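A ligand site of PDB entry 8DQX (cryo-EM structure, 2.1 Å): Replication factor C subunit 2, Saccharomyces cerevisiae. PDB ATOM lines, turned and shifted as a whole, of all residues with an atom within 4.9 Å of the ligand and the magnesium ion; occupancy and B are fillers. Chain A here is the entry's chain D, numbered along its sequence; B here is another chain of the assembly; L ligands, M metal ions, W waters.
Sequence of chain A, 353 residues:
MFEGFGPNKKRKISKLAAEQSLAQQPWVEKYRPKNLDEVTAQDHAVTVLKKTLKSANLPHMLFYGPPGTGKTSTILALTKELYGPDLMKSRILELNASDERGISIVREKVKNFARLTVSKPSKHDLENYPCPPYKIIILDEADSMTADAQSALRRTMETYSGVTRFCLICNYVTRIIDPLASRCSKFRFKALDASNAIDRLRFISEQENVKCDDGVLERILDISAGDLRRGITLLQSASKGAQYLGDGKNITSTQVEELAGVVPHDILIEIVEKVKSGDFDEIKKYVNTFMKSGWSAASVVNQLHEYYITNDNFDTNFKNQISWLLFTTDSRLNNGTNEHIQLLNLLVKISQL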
ATOM      1  N   TRP A  27       7.426   8.013  10.255  1.00  0.00           N
ATOM      2  CA  TRP A  27       6.946   6.816   9.594  1.00  0.00           C
ATOM      3  C   TRP A  27       5.546   6.410  10.055  1.00  0.00           C
ATOM      4  O   TRP A  27       4.779   5.835   9.279  1.00  0.00           O
ATOM      5  CB  TRP A  27       7.933   5.665   9.834  1.00  0.00           C
ATOM      6  CG  TRP A  27       9.214   5.816   9.059  1.00  0.00           C
ATOM      7  CD1 TRP A  27       9.618   6.905   8.344  1.00  0.00           C
ATOM      8  CD2 TRP A  27      10.264   4.853   8.945  1.00  0.00           C
ATOM      9  NE1 TRP A  27      10.858   6.677   7.783  1.00  0.00           N
ATOM     10  CE2 TRP A  27      11.274   5.426   8.141  1.00  0.00           C
ATOM     11  CE3 TRP A  27      10.459   3.559   9.448  1.00  0.00           C
ATOM     12  CZ2 TRP A  27      12.455   4.748   7.826  1.00  0.00           C
ATOM     13  CZ3 TRP A  27      11.625   2.898   9.130  1.00  0.00           C
ATOM     14  CH2 TRP A  27      12.613   3.493   8.325  1.00  0.00           C
ATOM     15  N   VAL A  28       5.182   6.719  11.313  1.00  0.00           N
ATOM     16  CA  VAL A  28       3.860   6.315  11.798  1.00  0.00           C
ATOM     17  C   VAL A  28       2.766   7.007  10.989  1.00  0.00           C
ATOM     18  O   VAL A  28       1.763   6.384  10.630  1.00  0.00           O
ATOM     19  CB  VAL A  28       3.710   6.596  13.306  1.00  0.00           C
ATOM     20  CG1 VAL A  28       4.477   5.563  14.114  1.00  0.00           C
ATOM     21  CG2 VAL A  28       4.150   8.022  13.676  1.00  0.00           C
ATOM     22  N   GLU A  29       2.941   8.293  10.681  1.00  0.00           N
ATOM     23  CA  GLU A  29       1.982   8.990   9.830  1.00  0.00           C
ATOM     24  C   GLU A  29       2.204   8.688   8.345  1.00  0.00           C
ATOM     25  O   GLU A  29       1.249   8.658   7.573  1.00  0.00           O
ATOM     26  CB  GLU A  29       2.053  10.496  10.070  1.00  0.00           C
ATOM     27  CG  GLU A  29       1.903  10.915  11.531  1.00  0.00           C
ATOM     28  CD  GLU A  29       0.709  10.272  12.238  1.00  0.00           C
ATOM     29  OE1 GLU A  29       0.736  10.194  13.486  1.00  0.00           O
ATOM     30  OE2 GLU A  29      -0.255   9.859  11.557  1.00  0.00           O
ATOM     31  N   TYR A  31       2.998   5.893   6.911  1.00  0.00           N
ATOM     32  CA  TYR A  31       2.467   4.581   6.549  1.00  0.00           C
ATOM     33  C   TYR A  31       1.104   4.323   7.187  1.00  0.00           C
ATOM     34  O   TYR A  31       0.725   3.177   7.394  1.00  0.00           O
ATOM     35  CB  TYR A  31       3.461   3.493   6.927  1.00  0.00           C
ATOM     36  CG  TYR A  31       4.721   3.543   6.096  1.00  0.00           C
ATOM     37  CD1 TYR A  31       4.761   2.968   4.828  1.00  0.00           C
ATOM     38  CD2 TYR A  31       5.863   4.176   6.559  1.00  0.00           C
ATOM     39  CE1 TYR A  31       5.913   3.023   4.054  1.00  0.00           C
ATOM     40  CE2 TYR A  31       7.021   4.234   5.797  1.00  0.00           C
ATOM     41  CZ  TYR A  31       7.032   3.649   4.546  1.00  0.00           C
ATOM     42  OH  TYR A  31       8.170   3.700   3.781  1.00  0.00           O
ATOM     43  N   ARG A  32       0.362   5.386   7.490  1.00  0.00           N
ATOM     44  CA  ARG A  32      -1.015   5.221   7.918  1.00  0.00           C
ATOM     45  C   ARG A  32      -1.818   4.560   6.796  1.00  0.00           C
ATOM     46  O   ARG A  32      -1.726   4.993   5.642  1.00  0.00           O
ATOM     47  CB  ARG A  32      -1.641   6.568   8.282  1.00  0.00           C
ATOM     48  CG  ARG A  32      -2.869   6.435   9.164  1.00  0.00           C
ATOM     49  CD  ARG A  32      -3.527   7.779   9.407  1.00  0.00           C
ATOM     50  NE  ARG A  32      -3.008   8.421  10.597  1.00  0.00           N
ATOM     51  CZ  ARG A  32      -3.209   7.994  11.841  1.00  0.00           C
ATOM     52  NH1 ARG A  32      -3.964   6.944  12.090  1.00  0.00           N
ATOM     53  NH2 ARG A  32      -2.644   8.645  12.848  1.00  0.00           N
ATOM     54  N   PRO A  33      -2.602   3.521   7.083  1.00  0.00           N
ATOM     55  CA  PRO A  33      -3.401   2.884   6.026  1.00  0.00           C
ATOM     56  C   PRO A  33      -4.260   3.890   5.283  1.00  0.00           C
ATOM     57  O   PRO A  33      -4.927   4.728   5.890  1.00  0.00           O
ATOM     58  CB  PRO A  33      -4.250   1.865   6.794  1.00  0.00           C
ATOM     59  CG  PRO A  33      -3.564   1.641   8.087  1.00  0.00           C
ATOM     60  CD  PRO A  33      -2.719   2.826   8.382  1.00  0.00           C
ATOM     61  N   GLU A  38      -5.658  -2.036   3.783  1.00  0.00           N
ATOM     62  CA  GLU A  38      -4.339  -1.836   4.369  1.00  0.00           C
ATOM     63  C   GLU A  38      -4.318  -2.074   5.885  1.00  0.00           C
ATOM     64  O   GLU A  38      -3.234  -2.225   6.455  1.00  0.00           O
ATOM     65  CB  GLU A  38      -3.839  -0.414   4.068  1.00  0.00           C
ATOM     66  CG  GLU A  38      -3.365  -0.196   2.641  1.00  0.00           C
ATOM     67  CD  GLU A  38      -2.077   0.589   2.581  1.00  0.00           C
ATOM     68  OE1 GLU A  38      -2.152   1.832   2.483  1.00  0.00           O
ATOM     69  OE2 GLU A  38      -0.995  -0.019   2.649  1.00  0.00           O
ATOM     70  N   VAL A  39      -5.475  -2.100   6.540  1.00  0.00           N
ATOM     71  CA  VAL A  39      -5.542  -2.483   7.947  1.00  0.00           C
ATOM     72  C   VAL A  39      -5.261  -3.973   8.055  1.00  0.00           C
ATOM     73  O   VAL A  39      -5.875  -4.789   7.357  1.00  0.00           O
ATOM     74  CB  VAL A  39      -6.904  -2.124   8.545  1.00  0.00           C
ATOM     75  CG1 VAL A  39      -6.956  -2.425  10.033  1.00  0.00           C
ATOM     76  CG2 VAL A  39      -7.242  -0.664   8.271  1.00  0.00           C
ATOM     77  N   THR A  40      -4.336  -4.351   8.950  1.00  0.00           N
ATOM     78  CA  THR A  40      -3.704  -5.659   8.811  1.00  0.00           C
ATOM     79  C   THR A  40      -4.403  -6.798   9.558  1.00  0.00           C
ATOM     80  O   THR A  40      -4.696  -7.837   8.957  1.00  0.00           O
ATOM     81  CB  THR A  40      -2.218  -5.584   9.220  1.00  0.00           C
ATOM     82  OG1 THR A  40      -1.614  -6.865   9.017  1.00  0.00           O
ATOM     83  CG2 THR A  40      -2.034  -5.161  10.673  1.00  0.00           C
ATOM     84  N   ALA A  41      -4.689  -6.641  10.857  1.00  0.00           N
ATOM     85  CA  ALA A  41      -5.057  -7.788  11.688  1.00  0.00           C
ATOM     86  C   ALA A  41      -6.429  -7.653  12.350  1.00  0.00           C
ATOM     87  O   ALA A  41      -6.676  -8.285  13.370  1.00  0.00           O
ATOM     88  CB  ALA A  41      -3.989  -8.026  12.745  1.00  0.00           C
ATOM     89  N   GLN A  42      -7.332  -6.849  11.789  1.00  0.00           N
ATOM     90  CA  GLN A  42      -8.649  -6.645  12.373  1.00  0.00           C
ATOM     91  C   GLN A  42      -9.744  -7.096  11.411  1.00  0.00           C
ATOM     92  O   GLN A  42     -10.791  -6.450  11.283  1.00  0.00           O
ATOM     93  CB  GLN A  42      -8.836  -5.189  12.788  1.00  0.00           C
ATOM     94  CG  GLN A  42      -7.614  -4.545  13.409  1.00  0.00           C
ATOM     95  CD  GLN A  42      -7.335  -5.031  14.825  1.00  0.00           C
ATOM     96  OE1 GLN A  42      -8.091  -5.822  15.377  1.00  0.00           O
ATOM     97  NE2 GLN A  42      -6.245  -4.553  15.415  1.00  0.00           N
ATOM     98  N   GLY A  65     -10.260  -0.477  22.028  1.00  0.00           N
ATOM     99  CA  GLY A  65      -9.096  -1.327  22.163  1.00  0.00           C
ATOM    100  C   GLY A  65      -7.846  -0.594  22.594  1.00  0.00           C
ATOM    101  O   GLY A  65      -7.828   0.637  22.743  1.00  0.00           O
ATOM    102  N   PRO A  66      -6.760  -1.337  22.788  1.00  0.00           N
ATOM    103  CA  PRO A  66      -5.534  -0.744  23.353  1.00  0.00           C
ATOM    104  C   PRO A  66      -4.828   0.156  22.345  1.00  0.00           C
ATOM    105  O   PRO A  66      -5.164   0.158  21.150  1.00  0.00           O
ATOM    106  CB  PRO A  66      -4.687  -1.973  23.711  1.00  0.00           C
ATOM    107  CG  PRO A  66      -5.133  -3.013  22.759  1.00  0.00           C
ATOM    108  CD  PRO A  66      -6.614  -2.793  22.592  1.00  0.00           C
ATOM    109  N   PRO A  67      -3.836   0.925  22.792  1.00  0.00           N
ATOM    110  CA  PRO A  67      -3.225   1.941  21.924  1.00  0.00           C
ATOM    111  C   PRO A  67      -2.585   1.377  20.672  1.00  0.00           C
ATOM    112  O   PRO A  67      -2.046   0.264  20.654  1.00  0.00           O
ATOM    113  CB  PRO A  67      -2.175   2.592  22.833  1.00  0.00           C
ATOM    114  CG  PRO A  67      -2.441   2.123  24.212  1.00  0.00           C
ATOM    115  CD  PRO A  67      -3.240   0.878  24.143  1.00  0.00           C
ATOM    116  N   GLY A  68      -2.657   2.165  19.601  1.00  0.00           N
ATOM    117  CA  GLY A  68      -1.940   1.868  18.372  1.00  0.00           C
ATOM    118  C   GLY A  68      -2.343   0.577  17.690  1.00  0.00           C
ATOM    119  O   GLY A  68      -1.480  -0.140  17.172  1.00  0.00           O
ATOM    120  N   THR A  69      -3.636   0.266  17.680  1.00  0.00           N
ATOM    121  CA  THR A  69      -4.130  -0.952  17.064  1.00  0.00           C
ATOM    122  C   THR A  69      -4.909  -0.710  15.768  1.00  0.00           C
ATOM    123  O   THR A  69      -5.188  -1.682  15.055  1.00  0.00           O
ATOM    124  CB  THR A  69      -5.012  -1.743  18.044  1.00  0.00           C
ATOM    125  OG1 THR A  69      -6.025  -0.893  18.590  1.00  0.00           O
ATOM    126  CG2 THR A  69      -4.166  -2.326  19.176  1.00  0.00           C
ATOM    127  N   GLY A  70      -5.269   0.529  15.448  1.00  0.00           N
ATOM    128  CA  GLY A  70      -5.825   0.852  14.145  1.00  0.00           C
ATOM    129  C   GLY A  70      -7.232   1.416  14.123  1.00  0.00           C
ATOM    130  O   GLY A  70      -7.889   1.401  13.072  1.00  0.00           O
ATOM    131  N   LYS A  71      -7.711   1.937  15.256  1.00  0.00           N
ATOM    132  CA  LYS A  71      -9.093   2.400  15.342  1.00  0.00           C
ATOM    133  C   LYS A  71      -9.300   3.685  14.528  1.00  0.00           C
ATOM    134  O   LYS A  71     -10.172   3.744  13.642  1.00  0.00           O
ATOM    135  CB  LYS A  71      -9.471   2.597  16.812  1.00  0.00           C
ATOM    136  CG  LYS A  71      -9.163   1.377  17.688  1.00  0.00           C
ATOM    137  CD  LYS A  71      -9.603   1.551  19.148  1.00  0.00           C
ATOM    138  CE  LYS A  71      -8.761   2.582  19.889  1.00  0.00           C
ATOM    139  NZ  LYS A  71      -7.325   2.199  19.993  1.00  0.00           N
ATOM    140  N   THR A  72      -8.502   4.718  14.808  1.00  0.00           N
ATOM    141  CA  THR A  72      -8.625   5.975  14.069  1.00  0.00           C
ATOM    142  C   THR A  72      -8.352   5.753  12.587  1.00  0.00           C
ATOM    143  O   THR A  72      -9.087   6.270  11.722  1.00  0.00           O
ATOM    144  CB  THR A  72      -7.659   7.017  14.650  1.00  0.00           C
ATOM    145  OG1 THR A  72      -8.092   7.377  15.974  1.00  0.00           O
ATOM    146  CG2 THR A  72      -7.601   8.271  13.790  1.00  0.00           C
ATOM    147  N   SER A  73      -7.321   4.973  12.270  1.00  0.00           N
ATOM    148  CA  SER A  73      -7.023   4.657  10.878  1.00  0.00           C
ATOM    149  C   SER A  73      -8.229   4.009  10.200  1.00  0.00           C
ATOM    150  O   SER A  73      -8.579   4.359   9.074  1.00  0.00           O
ATOM    151  CB  SER A  73      -5.806   3.734  10.804  1.00  0.00           C
ATOM    152  OG  SER A  73      -4.695   4.305  11.469  1.00  0.00           O
ATOM    153  N   ASP A 140     -13.940  10.663  18.488  1.00  0.00           N
ATOM    154  CA  ASP A 140     -12.700  10.003  18.850  1.00  0.00           C
ATOM    155  C   ASP A 140     -12.354  10.315  20.297  1.00  0.00           C
ATOM    156  O   ASP A 140     -12.622  11.421  20.784  1.00  0.00           O
ATOM    157  CB  ASP A 140     -11.557  10.416  17.920  1.00  0.00           C
ATOM    158  CG  ASP A 140     -10.479   9.349  17.781  1.00  0.00           C
ATOM    159  OD1 ASP A 140     -10.501   8.362  18.553  1.00  0.00           O
ATOM    160  OD2 ASP A 140      -9.599   9.491  16.914  1.00  0.00           O
ATOM    161  N   GLU A 141     -11.751   9.349  20.982  1.00  0.00           N
ATOM    162  CA  GLU A 141     -11.401   9.497  22.398  1.00  0.00           C
ATOM    163  C   GLU A 141     -12.648   9.830  23.226  1.00  0.00           C
ATOM    164  O   GLU A 141     -12.630  10.707  24.093  1.00  0.00           O
ATOM    165  CB  GLU A 141     -10.312  10.555  22.581  1.00  0.00           C
ATOM    166  CG  GLU A 141      -8.962  10.129  22.029  1.00  0.00           C
ATOM    167  CD  GLU A 141      -8.302  11.175  21.120  1.00  0.00           C
ATOM    168  OE1 GLU A 141      -8.791  12.317  21.063  1.00  0.00           O
ATOM    169  OE2 GLU A 141      -7.295  10.843  20.478  1.00  0.00           O
ATOM    170  N   ASN A 171     -10.216   3.712  24.312  1.00  0.00           N
ATOM    171  CA  ASN A 171      -9.309   2.705  24.858  1.00  0.00           C
ATOM    172  C   ASN A 171      -9.895   1.972  26.050  1.00  0.00           C
ATOM    173  O   ASN A 171      -9.592   0.796  26.256  1.00  0.00           O
ATOM    174  CB  ASN A 171      -7.975   3.350  25.271  1.00  0.00           C
ATOM    175  CG  ASN A 171      -7.228   3.978  24.097  1.00  0.00           C
ATOM    176  OD1 ASN A 171      -7.062   5.193  24.030  1.00  0.00           O
ATOM    177  ND2 ASN A 171      -6.765   3.145  23.173  1.00  0.00           N
ATOM    178  N   LEU A 192      -1.735  -6.120  18.556  1.00  0.00           N
ATOM    179  CA  LEU A 192      -0.931  -6.488  17.393  1.00  0.00           C
ATOM    180  C   LEU A 192       0.419  -7.019  17.847  1.00  0.00           C
ATOM    181  O   LEU A 192       1.181  -6.297  18.503  1.00  0.00           O
ATOM    182  CB  LEU A 192      -0.762  -5.278  16.458  1.00  0.00           C
ATOM    183  CG  LEU A 192      -2.076  -4.635  16.000  1.00  0.00           C
ATOM    184  CD1 LEU A 192      -1.808  -3.435  15.104  1.00  0.00           C
ATOM    185  CD2 LEU A 192      -2.941  -5.643  15.292  1.00  0.00           C
ATOM    186  N   ARG A 200       3.029  -6.522   7.940  1.00  0.00           N
ATOM    187  CA  ARG A 200       3.016  -5.076   7.747  1.00  0.00           C
ATOM    188  C   ARG A 200       4.358  -4.459   8.137  1.00  0.00           C
ATOM    189  O   ARG A 200       4.873  -3.586   7.435  1.00  0.00           O
ATOM    190  CB  ARG A 200       1.880  -4.447   8.555  1.00  0.00           C
ATOM    191  CG  ARG A 200       1.748  -2.934   8.403  1.00  0.00           C
ATOM    192  CD  ARG A 200       1.488  -2.528   6.963  1.00  0.00           C
ATOM    193  NE  ARG A 200       1.184  -1.108   6.834  1.00  0.00           N
ATOM    194  CZ  ARG A 200       0.904  -0.497   5.694  1.00  0.00           C
ATOM    195  NH1 ARG A 200       0.881  -1.154   4.543  1.00  0.00           N
ATOM    196  NH2 ARG A 200       0.652   0.810   5.702  1.00  0.00           N
ATOM    197  N   LEU A 228       1.404  -1.271  17.456  1.00  0.00           N
ATOM    198  CA  LEU A 228       2.150  -1.206  16.203  1.00  0.00           C
ATOM    199  C   LEU A 228       2.736   0.187  15.944  1.00  0.00           C
ATOM    200  O   LEU A 228       3.775   0.296  15.293  1.00  0.00           O
ATOM    201  CB  LEU A 228       1.256  -1.615  15.041  1.00  0.00           C
ATOM    202  CG  LEU A 228       1.878  -1.656  13.642  1.00  0.00           C
ATOM    203  CD1 LEU A 228       3.216  -2.377  13.637  1.00  0.00           C
ATOM    204  CD2 LEU A 228       0.915  -2.295  12.650  1.00  0.00           C
ATOM    205  N   ARG A 229       2.095   1.249  16.454  1.00  0.00           N
ATOM    206  CA  ARG A 229       2.687   2.575  16.362  1.00  0.00           C
ATOM    207  C   ARG A 229       4.071   2.593  17.020  1.00  0.00           C
ATOM    208  O   ARG A 229       5.050   3.091  16.445  1.00  0.00           O
ATOM    209  CB  ARG A 229       1.767   3.609  17.013  1.00  0.00           C
ATOM    210  CG  ARG A 229       2.193   5.054  16.821  1.00  0.00           C
ATOM    211  CD  ARG A 229       1.496   5.991  17.790  1.00  0.00           C
ATOM    212  NE  ARG A 229       0.114   6.299  17.411  1.00  0.00           N
ATOM    213  CZ  ARG A 229      -0.960   5.917  18.093  1.00  0.00           C
ATOM    214  NH1 ARG A 229      -0.874   5.146  19.160  1.00  0.00           N
ATOM    215  NH2 ARG A 229      -2.162   6.328  17.684  1.00  0.00           N
ATOM    216  N   ILE A 232       6.670   0.663  14.893  1.00  0.00           N
ATOM    217  CA  ILE A 232       7.148   1.415  13.730  1.00  0.00           C
ATOM    218  C   ILE A 232       8.115   2.505  14.168  1.00  0.00           C
ATOM    219  O   ILE A 232       9.147   2.733  13.527  1.00  0.00           O
ATOM    220  CB  ILE A 232       5.961   1.991  12.923  1.00  0.00           C
ATOM    221  CG1 ILE A 232       5.100   0.853  12.365  1.00  0.00           C
ATOM    222  CG2 ILE A 232       6.480   2.876  11.798  1.00  0.00           C
ATOM    223  CD1 ILE A 232       3.778   1.329  11.777  1.00  0.00           C
ATOM    224  N   ARG B 155      -3.354  14.285  22.003  1.00  0.00           N
ATOM    225  CA  ARG B 155      -3.213  13.076  21.206  1.00  0.00           C
ATOM    226  C   ARG B 155      -3.407  13.339  19.712  1.00  0.00           C
ATOM    227  O   ARG B 155      -2.542  12.990  18.898  1.00  0.00           O
ATOM    228  CB  ARG B 155      -4.214  12.015  21.681  1.00  0.00           C
ATOM    229  CG  ARG B 155      -3.852  11.374  23.005  1.00  0.00           C
ATOM    230  CD  ARG B 155      -5.014  10.596  23.585  1.00  0.00           C
ATOM    231  NE  ARG B 155      -5.445   9.508  22.709  1.00  0.00           N
ATOM    232  CZ  ARG B 155      -6.154   8.464  23.104  1.00  0.00           C
ATOM    233  NH1 ARG B 155      -6.520   8.304  24.369  1.00  0.00           N
ATOM    234  NH2 ARG B 155      -6.501   7.536  22.213  1.00  0.00           N
ATOM    235  N   GLU B 159      -0.890  13.945  15.843  1.00  0.00           N
ATOM    236  CA  GLU B 159      -0.995  13.157  14.610  1.00  0.00           C
ATOM    237  C   GLU B 159      -1.435  13.990  13.417  1.00  0.00           C
ATOM    238  O   GLU B 159      -0.835  13.924  12.346  1.00  0.00           O
ATOM    239  CB  GLU B 159      -1.983  12.002  14.812  1.00  0.00           C
ATOM    240  CG  GLU B 159      -1.582  11.030  15.910  1.00  0.00           C
ATOM    241  CD  GLU B 159      -2.500   9.832  15.961  1.00  0.00           C
ATOM    242  OE1 GLU B 159      -3.695  10.013  16.271  1.00  0.00           O
ATOM    243  OE2 GLU B 159      -2.024   8.711  15.676  1.00  0.00           O
ATOM    244  N   PRO B 180      -1.341   6.302  25.714  1.00  0.00           N
ATOM    245  CA  PRO B 180      -1.411   6.831  24.340  1.00  0.00           C
ATOM    246  C   PRO B 180      -0.349   7.866  24.018  1.00  0.00           C
ATOM    247  O   PRO B 180       0.104   7.935  22.866  1.00  0.00           O
ATOM    248  CB  PRO B 180      -2.832   7.433  24.268  1.00  0.00           C
ATOM    249  CG  PRO B 180      -3.611   6.685  25.290  1.00  0.00           C
ATOM    250  CD  PRO B 180      -2.639   6.369  26.400  1.00  0.00           C
ATOM    251  N   ARG B 184       2.971   7.650  21.217  1.00  0.00           N
ATOM    252  CA  ARG B 184       3.207   8.621  20.152  1.00  0.00           C
ATOM    253  C   ARG B 184       4.611   9.215  20.171  1.00  0.00           C
ATOM    254  O   ARG B 184       4.921  10.040  19.303  1.00  0.00           O
ATOM    255  CB  ARG B 184       2.190   9.769  20.240  1.00  0.00           C
ATOM    256  CG  ARG B 184       0.808   9.420  19.697  1.00  0.00           C
ATOM    257  CD  ARG B 184      -0.267  10.335  20.294  1.00  0.00           C
ATOM    258  NE  ARG B 184      -1.552  10.201  19.617  1.00  0.00           N
ATOM    259  CZ  ARG B 184      -2.409   9.217  19.841  1.00  0.00           C
ATOM    260  NH1 ARG B 184      -2.173   8.265  20.729  1.00  0.00           N
ATOM    261  NH2 ARG B 184      -3.543   9.193  19.148  1.00  0.00           N
HETATM  262  P1  LIG L   1      -5.030   5.280  20.047  1.00  0.00           P
HETATM  263  S1  LIG L   1      -3.634   5.381  21.368  1.00  0.00           S
HETATM  264  O1  LIG L   1      -5.438   6.814  19.564  1.00  0.00           O
HETATM  265  O2  LIG L   1      -6.384   4.507  20.640  1.00  0.00           O
HETATM  266  P2  LIG L   1      -5.224   3.992  17.426  1.00  0.00           P
HETATM  267  O3  LIG L   1      -5.948   2.678  17.644  1.00  0.00           O
HETATM  268  O4  LIG L   1      -6.209   5.069  16.989  1.00  0.00           O
HETATM  269  O5  LIG L   1      -4.410   4.468  18.772  1.00  0.00           O
HETATM  270  P3  LIG L   1      -3.984   4.472  14.880  1.00  0.00           P
HETATM  271  O6  LIG L   1      -5.146   4.009  14.055  1.00  0.00           O
HETATM  272  O7  LIG L   1      -3.981   5.971  14.986  1.00  0.00           O
HETATM  273  O8  LIG L   1      -4.062   3.778  16.322  1.00  0.00           O
HETATM  274  O9  LIG L   1      -2.546   3.923  14.218  1.00  0.00           O
HETATM  275  C1  LIG L   1      -1.366   4.566  14.543  1.00  0.00           C
HETATM  276  C2  LIG L   1      -0.309   4.143  13.576  1.00  0.00           C
HETATM  277  O10 LIG L   1       0.141   2.950  13.894  1.00  0.00           O
HETATM  278  C3  LIG L   1      -0.963   4.046  12.050  1.00  0.00           C
HETATM  279  O11 LIG L   1      -0.727   5.335  11.348  1.00  0.00           O
HETATM  280  C4  LIG L   1      -0.368   3.092  11.500  1.00  0.00           C
HETATM  281  O12 LIG L   1       0.932   3.538  10.936  1.00  0.00           O
HETATM  282  C5  LIG L   1      -0.073   2.062  12.693  1.00  0.00           C
HETATM  283  N1  LIG L   1      -1.051   1.196  12.948  1.00  0.00           N
HETATM  284  C6  LIG L   1      -1.753   0.925  14.042  1.00  0.00           C
HETATM  285  N2  LIG L   1      -2.604  -0.048  13.777  1.00  0.00           N
HETATM  286  C7  LIG L   1      -2.434  -0.412  12.506  1.00  0.00           C
HETATM  287  C8  LIG L   1      -3.053  -1.366  11.735  1.00  0.00           C
HETATM  288  N3  LIG L   1      -4.125  -2.276  12.156  1.00  0.00           N
HETATM  289  N4  LIG L   1      -2.683  -1.534  10.475  1.00  0.00           N
HETATM  290  C9  LIG L   1      -1.714  -0.760   9.959  1.00  0.00           C
HETATM  291  N5  LIG L   1      -1.115   0.174  10.721  1.00  0.00           N
HETATM  292  C10 LIG L   1      -1.479   0.345  11.993  1.00  0.00           C
HETATM  293 MG    MG M   1      -6.494   6.864  17.929  1.00  0.00          MG
HETATM  294  O   HOH W   1      -5.221   0.334  10.764  1.00  0.00           O
HETATM  295  O   HOH W   2      -7.144   9.159  18.512  1.00  0.00           O
HETATM  296  O   HOH W   3       1.029   0.638   9.091  1.00  0.00           O
HETATM  297  O   HOH W   4      -8.826   5.384  21.558  1.00  0.00           O
HETATM  298  O   HOH W   5      -4.772   7.525  16.573  1.00  0.00           O
HETATM  299  O   HOH W   6      -8.435   6.321  19.041  1.00  0.00           O
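The side-chain hydroxyl of Ser 73 lies within hydrogen-bond range of an oxygen (O6) of the ligand (2.6 Å).
The backbone NH of Thr 69 lies within hydrogen-bond range of an oxygen (O3) of the ligand.
N of Thr 72 sits close to O4 of the ligand (3.2 Å).
An oxygen (O7) of the ligand lies within salt-bridge range of the guanidinium group of Arg 229.
The backbone NH (N) of Lys 71 is in hydrogen-bond range of an oxygen (O3) of the ligand (3.1 Å).
The backbone carbonyl oxygen of Thr 69 is in hydrogen-bond range of a nitrogen (N3) of the ligand (3.1 Å).
An oxygen (O2) of the ligand lies within hydrogen-bond range of the side-chain amide nitrogen (ND2) of Asn 171 (2.9 Å).
The guanidinium group (NH1) of Arg 184 of chain B lies close to a sulfur (S1) of the ligand.
The backbone NH (N) of Gly 68 lies within hydrogen-bond range of an oxygen (O5) of the ligand (3.0 Å).
The guanidinium group of Arg 32 lies within salt-bridge range of an oxygen (O7) of the ligand.
N of Ser 73 is in hydrogen-bond range of O6 of the ligand.
NZ of Lys 71 lies within salt-bridge range of O3 of the ligand.
The backbone NH (N) of Gly 70 sits at hydrogen-bond distance from an oxygen (O3) of the ligand, at 3.1 Å.
O of Val 28 sits at hydrogen-bond distance from O11 of the ligand (2.8 Å).
The guanidinium group (NH2) of Arg 155 of chain B sits at hydrogen-bond distance from an oxygen (O2) of the ligand, at 3.4 Å.
The side-chain amino group (NZ) of Lys 71 is in hydrogen-bond range of the backbone carbonyl oxygen (O) of Pro 66.
The side-chain carboxylate (OE2) of Glu 159 of chain B is in salt-bridge range of the guanidinium group (NH2) of Arg 32 (2.9 Å).
The guanidinium group (NH1) of Arg 184 of chain B lies within hydrogen-bond range of the backbone carbonyl oxygen (O) of Pro 180 of chain B (3.1 Å).
O of Tyr 31 lies within hydrogen-bond range of NH2 of Arg 200.
O of Gly 65 sits at hydrogen-bond distance from ND2 of Asn 171, at 2.8 Å.
N of Leu 228 sits at hydrogen-bond distance from O of Gly 68, at 3.1 Å.
ND2 of Asn 171 lies close to NZ of Lys 71, at 3.4 Å.
The side-chain hydroxyl (OG1) of Thr 69 is in hydrogen-bond range of the backbone carbonyl oxygen (O) of Pro 66, at 2.9 Å.
OE2 of Glu 159 of chain B sits close to O7 of the ligand (3.4 Å).
Merely in contact with the ligand: Tyr 31, Pro 33, Val 39, Thr 40, Pro 67, Leu 192, Leu 228, Ile 232 and Pro 180 of chain B.
Hydrophobic or aromatic side chains that line the ligand: Pro 33, Val 39, Pro 67, Leu 192, Leu 228, Ile 232 and Pro 180 of chain B.
Of the 32 residues printed, 22 come within 4 Å of the ligand.
The nearest printed residue that does not touch the ligand is Glu 38 (4.1 Å).
Arg 184 of chain B touches the magnesium ion (NH2 to MG, 3.95 Å).
Of the 32 residues printed, 2 come within 4 Å of the magnesium ion.
The magnesium ion is bound by an oxygen (O1) of the ligand (1.9 Å), an oxygen (O4) of the ligand (2.0 Å), water W5 (2.3 Å), water W6 (2.3 Å), water W2 (2.5 Å) and the side-chain hydroxyl of Thr 72 (2.6 Å).
Water W6 lies within hydrogen-bond range of the side-chain carboxylate of Asp 140 and an oxygen (O2) of the ligand.
Water W2 lies within hydrogen-bond range of OE2 of Glu 141 (2.6 Å) and OD2 of Asp 140 (2.9 Å).
Water W5 lies within hydrogen-bond range of the side-chain carboxylate (OE1) of Glu 159 of chain B (2.7 Å), the guanidinium group (NH2) of Arg 229 (3.1 Å) and the guanidinium group (NH2) of Arg 184 of chain B (3.3 Å).
Water W3 lies within hydrogen-bond range of a nitrogen (N5) of the ligand (2.7 Å), the guanidinium group of Arg 200 (2.9 Å) and the backbone carbonyl oxygen of Tyr 31 (3.1 Å).
Water W4 lies within hydrogen-bond range of O2 of the ligand (2.8 Å), OD1 of Asn 171 (3.0 Å) and NH2 of Arg 155 of chain B (3.2 Å).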
